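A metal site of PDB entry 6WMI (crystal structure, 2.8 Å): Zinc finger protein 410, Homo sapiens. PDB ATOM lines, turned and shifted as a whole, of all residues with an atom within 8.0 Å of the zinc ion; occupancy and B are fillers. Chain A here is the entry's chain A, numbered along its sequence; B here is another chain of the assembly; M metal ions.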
ATOM      1  N   ILE A  39      16.396   1.299 -19.973  1.00  0.00           N
ATOM      2  CA  ILE A  39      17.722   0.718 -20.104  1.00  0.00           C
ATOM      3  C   ILE A  39      17.620  -0.776 -20.333  1.00  0.00           C
ATOM      4  O   ILE A  39      16.874  -1.472 -19.639  1.00  0.00           O
ATOM      5  CB  ILE A  39      18.574   1.015 -18.855  1.00  0.00           C
ATOM      6  CG1 ILE A  39      18.632   2.524 -18.612  1.00  0.00           C
ATOM      7  CG2 ILE A  39      19.948   0.405 -19.003  1.00  0.00           C
ATOM      8  CD1 ILE A  39      19.447   2.929 -17.411  1.00  0.00           C
ATOM      9  N   CYS A  40      18.402  -1.285 -21.299  1.00  0.00           N
ATOM     10  CA  CYS A  40      18.427  -2.714 -21.585  1.00  0.00           C
ATOM     11  C   CYS A  40      19.107  -3.468 -20.446  1.00  0.00           C
ATOM     12  O   CYS A  40      20.248  -3.138 -20.085  1.00  0.00           O
ATOM     13  CB  CYS A  40      19.152  -2.985 -22.910  1.00  0.00           C
ATOM     14  SG  CYS A  40      19.421  -4.746 -23.309  1.00  0.00           S
ATOM     15  N   PRO A  41      18.458  -4.490 -19.879  1.00  0.00           N
ATOM     16  CA  PRO A  41      19.054  -5.227 -18.750  1.00  0.00           C
ATOM     17  C   PRO A  41      19.989  -6.361 -19.140  1.00  0.00           C
ATOM     18  O   PRO A  41      20.604  -6.955 -18.244  1.00  0.00           O
ATOM     19  CB  PRO A  41      17.811  -5.778 -18.041  1.00  0.00           C
ATOM     20  CG  PRO A  41      16.855  -6.046 -19.167  1.00  0.00           C
ATOM     21  CD  PRO A  41      17.105  -4.966 -20.192  1.00  0.00           C
ATOM     22  N   ALA A  42      20.113  -6.687 -20.425  1.00  0.00           N
ATOM     23  CA  ALA A  42      21.032  -7.731 -20.848  1.00  0.00           C
ATOM     24  C   ALA A  42      22.467  -7.361 -20.479  1.00  0.00           C
ATOM     25  O   ALA A  42      22.861  -6.191 -20.526  1.00  0.00           O
ATOM     26  CB  ALA A  42      20.920  -7.961 -22.357  1.00  0.00           C
ATOM     27  N   GLU A  43      23.256  -8.369 -20.103  1.00  0.00           N
ATOM     28  CA  GLU A  43      24.609  -8.118 -19.621  1.00  0.00           C
ATOM     29  C   GLU A  43      25.512  -7.681 -20.766  1.00  0.00           C
ATOM     30  O   GLU A  43      25.535  -8.312 -21.826  1.00  0.00           O
ATOM     31  CB  GLU A  43      25.179  -9.370 -18.950  1.00  0.00           C
ATOM     32  N   GLY A  44      26.246  -6.593 -20.553  1.00  0.00           N
ATOM     33  CA  GLY A  44      27.207  -6.102 -21.513  1.00  0.00           C
ATOM     34  C   GLY A  44      26.665  -5.141 -22.554  1.00  0.00           C
ATOM     35  O   GLY A  44      27.456  -4.603 -23.339  1.00  0.00           O
ATOM     36  N   CYS A  45      25.354  -4.908 -22.593  1.00  0.00           N
ATOM     37  CA  CYS A  45      24.779  -4.033 -23.615  1.00  0.00           C
ATOM     38  C   CYS A  45      24.684  -2.585 -23.136  1.00  0.00           C
ATOM     39  O   CYS A  45      25.364  -1.701 -23.670  1.00  0.00           O
ATOM     40  CB  CYS A  45      23.398  -4.546 -24.026  1.00  0.00           C
ATOM     41  SG  CYS A  45      22.538  -3.557 -25.271  1.00  0.00           S
ATOM     42  N   GLY A  46      23.874  -2.338 -22.097  1.00  0.00           N
ATOM     43  CA  GLY A  46      23.764  -1.021 -21.512  1.00  0.00           C
ATOM     44  C   GLY A  46      23.214   0.069 -22.400  1.00  0.00           C
ATOM     45  O   GLY A  46      23.396   1.251 -22.114  1.00  0.00           O
ATOM     46  N   LYS A  47      22.524  -0.289 -23.488  1.00  0.00           N
ATOM     47  CA  LYS A  47      21.896   0.727 -24.314  1.00  0.00           C
ATOM     48  C   LYS A  47      20.604   1.223 -23.665  1.00  0.00           C
ATOM     49  O   LYS A  47      19.990   0.534 -22.841  1.00  0.00           O
ATOM     50  CB  LYS A  47      21.599   0.180 -25.714  1.00  0.00           C
ATOM     51  CG  LYS A  47      22.832  -0.058 -26.556  1.00  0.00           C
ATOM     52  CD  LYS A  47      22.476  -0.657 -27.912  1.00  0.00           C
ATOM     53  CE  LYS A  47      23.720  -1.163 -28.628  1.00  0.00           C
ATOM     54  NZ  LYS A  47      24.782  -0.124 -28.683  1.00  0.00           N
ATOM     55  N   SER A  48      20.199   2.429 -24.034  1.00  0.00           N
ATOM     56  CA  SER A  48      19.053   3.087 -23.420  1.00  0.00           C
ATOM     57  C   SER A  48      18.220   3.787 -24.471  1.00  0.00           C
ATOM     58  O   SER A  48      18.709   4.155 -25.545  1.00  0.00           O
ATOM     59  CB  SER A  48      19.495   4.092 -22.344  1.00  0.00           C
ATOM     60  OG  SER A  48      20.340   5.083 -22.906  1.00  0.00           O
ATOM     61  N   PHE A  49      16.941   3.997 -24.158  1.00  0.00           N
ATOM     62  CA  PHE A  49      15.968   4.442 -25.139  1.00  0.00           C
ATOM     63  C   PHE A  49      15.030   5.457 -24.512  1.00  0.00           C
ATOM     64  O   PHE A  49      14.896   5.546 -23.292  1.00  0.00           O
ATOM     65  CB  PHE A  49      15.194   3.245 -25.726  1.00  0.00           C
ATOM     66  CG  PHE A  49      16.088   2.180 -26.298  1.00  0.00           C
ATOM     67  CD1 PHE A  49      16.428   2.186 -27.641  1.00  0.00           C
ATOM     68  CD2 PHE A  49      16.610   1.181 -25.483  1.00  0.00           C
ATOM     69  CE1 PHE A  49      17.264   1.210 -28.168  1.00  0.00           C
ATOM     70  CE2 PHE A  49      17.446   0.205 -26.010  1.00  0.00           C
ATOM     71  CZ  PHE A  49      17.773   0.216 -27.356  1.00  0.00           C
ATOM     72  N   LEU A  55      12.702  -0.082 -26.316  1.00  0.00           N
ATOM     73  CA  LEU A  55      13.411  -1.122 -25.577  1.00  0.00           C
ATOM     74  C   LEU A  55      12.848  -2.497 -25.885  1.00  0.00           C
ATOM     75  O   LEU A  55      13.607  -3.459 -26.060  1.00  0.00           O
ATOM     76  CB  LEU A  55      13.339  -0.836 -24.081  1.00  0.00           C
ATOM     77  CG  LEU A  55      13.986  -1.881 -23.182  1.00  0.00           C
ATOM     78  CD1 LEU A  55      15.465  -1.977 -23.504  1.00  0.00           C
ATOM     79  CD2 LEU A  55      13.777  -1.513 -21.735  1.00  0.00           C
ATOM     80  N   HIS A  58      14.112  -3.519 -29.209  1.00  0.00           N
ATOM     81  CA  HIS A  58      15.543  -3.803 -29.107  1.00  0.00           C
ATOM     82  C   HIS A  58      15.801  -5.190 -28.535  1.00  0.00           C
ATOM     83  O   HIS A  58      16.772  -5.854 -28.933  1.00  0.00           O
ATOM     84  CB  HIS A  58      16.247  -2.756 -28.243  1.00  0.00           C
ATOM     85  CG  HIS A  58      17.645  -3.129 -27.862  1.00  0.00           C
ATOM     86  ND1 HIS A  58      18.721  -2.972 -28.710  1.00  0.00           N
ATOM     87  CD2 HIS A  58      18.144  -3.644 -26.717  1.00  0.00           C
ATOM     88  CE1 HIS A  58      19.821  -3.376 -28.113  1.00  0.00           C
ATOM     89  NE2 HIS A  58      19.505  -3.786 -26.895  1.00  0.00           N
ATOM     90  N   MET A  59      14.949  -5.653 -27.614  1.00  0.00           N
ATOM     91  CA  MET A  59      15.153  -6.971 -27.006  1.00  0.00           C
ATOM     92  C   MET A  59      15.215  -8.074 -28.058  1.00  0.00           C
ATOM     93  O   MET A  59      15.905  -9.084 -27.845  1.00  0.00           O
ATOM     94  CB  MET A  59      14.050  -7.285 -26.005  1.00  0.00           C
ATOM     95  CG  MET A  59      14.040  -6.364 -24.780  1.00  0.00           C
ATOM     96  SD  MET A  59      15.668  -6.078 -24.054  1.00  0.00           S
ATOM     97  CE  MET A  59      16.184  -7.734 -23.594  1.00  0.00           C
ATOM     98  N   ARG A  60      14.541  -7.890 -29.187  1.00  0.00           N
ATOM     99  CA  ARG A  60      14.559  -8.910 -30.228  1.00  0.00           C
ATOM    100  C   ARG A  60      15.957  -9.140 -30.787  1.00  0.00           C
ATOM    101  O   ARG A  60      16.191 -10.171 -31.428  1.00  0.00           O
ATOM    102  CB  ARG A  60      13.598  -8.524 -31.344  1.00  0.00           C
ATOM    103  CG  ARG A  60      12.145  -8.684 -30.943  1.00  0.00           C
ATOM    104  CD  ARG A  60      11.209  -8.014 -31.928  1.00  0.00           C
ATOM    105  NE  ARG A  60       9.848  -7.981 -31.416  1.00  0.00           N
ATOM    106  CZ  ARG A  60       8.918  -7.123 -31.834  1.00  0.00           C
ATOM    107  NH1 ARG A  60       9.230  -6.231 -32.772  1.00  0.00           N
ATOM    108  NH2 ARG A  60       7.700  -7.157 -31.312  1.00  0.00           N
ATOM    109  N   THR A  61      16.898  -8.221 -30.561  1.00  0.00           N
ATOM    110  CA  THR A  61      18.278  -8.475 -30.945  1.00  0.00           C
ATOM    111  C   THR A  61      18.995  -9.394 -29.970  1.00  0.00           C
ATOM    112  O   THR A  61      20.079  -9.892 -30.288  1.00  0.00           O
ATOM    113  CB  THR A  61      19.087  -7.162 -31.059  1.00  0.00           C
ATOM    114  OG1 THR A  61      19.043  -6.461 -29.810  1.00  0.00           O
ATOM    115  CG2 THR A  61      18.536  -6.281 -32.177  1.00  0.00           C
ATOM    116  N   HIS A  62      18.413  -9.641 -28.784  1.00  0.00           N
ATOM    117  CA  HIS A  62      19.006 -10.541 -27.806  1.00  0.00           C
ATOM    118  C   HIS A  62      18.295 -11.889 -27.733  1.00  0.00           C
ATOM    119  O   HIS A  62      18.947 -12.894 -27.418  1.00  0.00           O
ATOM    120  CB  HIS A  62      19.004  -9.911 -26.412  1.00  0.00           C
ATOM    121  CG  HIS A  62      19.835  -8.664 -26.292  1.00  0.00           C
ATOM    122  ND1 HIS A  62      21.169  -8.609 -26.655  1.00  0.00           N
ATOM    123  CD2 HIS A  62      19.532  -7.438 -25.794  1.00  0.00           C
ATOM    124  CE1 HIS A  62      21.632  -7.397 -26.417  1.00  0.00           C
ATOM    125  NE2 HIS A  62      20.676  -6.667 -25.893  1.00  0.00           N
ATOM    126  P    DT B  10      17.888  -1.593 -32.087  1.00  0.00           P
ATOM    127  OP1  DT B  10      18.744  -1.592 -30.882  1.00  0.00           O
ATOM    128  OP2  DT B  10      16.581  -2.286 -32.058  1.00  0.00           O
ATOM    129  O5'  DT B  10      17.658  -0.075 -32.496  1.00  0.00           O
ATOM    130  C5'  DT B  10      18.794   0.744 -32.685  1.00  0.00           C
ATOM    131  C4'  DT B  10      18.377   2.156 -33.066  1.00  0.00           C
ATOM    132  O4'  DT B  10      17.631   2.116 -34.307  1.00  0.00           O
ATOM    133  C3'  DT B  10      17.478   2.872 -32.056  1.00  0.00           C
ATOM    134  O3'  DT B  10      17.870   4.229 -32.023  1.00  0.00           O
ATOM    135  C2'  DT B  10      16.093   2.701 -32.679  1.00  0.00           C
ATOM    136  C1'  DT B  10      16.444   2.840 -34.142  1.00  0.00           C
ATOM    137  N1   DT B  10      15.430   2.305 -35.076  1.00  0.00           N
ATOM    138  C2   DT B  10      14.948   3.118 -36.064  1.00  0.00           C
ATOM    139  O2   DT B  10      15.299   4.275 -36.203  1.00  0.00           O
ATOM    140  N3   DT B  10      14.042   2.538 -36.900  1.00  0.00           N
ATOM    141  C4   DT B  10      13.568   1.242 -36.852  1.00  0.00           C
ATOM    142  O4   DT B  10      12.737   0.808 -37.642  1.00  0.00           O
ATOM    143  C5   DT B  10      14.115   0.427 -35.787  1.00  0.00           C
ATOM    144  C7   DT B  10      13.679  -0.993 -35.626  1.00  0.00           C
ATOM    145  C6   DT B  10      15.025   0.988 -34.961  1.00  0.00           C
HETATM  146 ZN    ZN M   1      20.541  -4.692 -25.401  1.00  0.00          ZN
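The side-chain sulfur of Cys 45 sits close to the backbone NH of Lys 47 (3.7 Å). The side-chain sulfur of Cys 40 lies close to the backbone NH of Ala 42, 3.5 Å away. OP1 of DT 10 of chain B lies within hydrogen-bond range of ND1 of His 58 (2.6 Å). The side-chain hydroxyl of Thr 61 sits at hydrogen-bond distance from the backbone carbonyl oxygen of His 58 (2.5 Å). O of Lys 47 lies within hydrogen-bond range of N of Cys 40.
Four residues have an atom within 4 Å of the zinc ion: Cys 40, Cys 45, His 58 and His 62.
NE2 of His 58 is bound to the zinc ion, at 2.0 Å. The zinc ion is bound by NE2 of His 62, 2.0 Å away. The zinc ion is bound by SG of Cys 45. The side-chain sulfur (SG) of Cys 40 is bound to the zinc ion (2.4 Å). The zinc ion has four donor atoms within binding distance.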
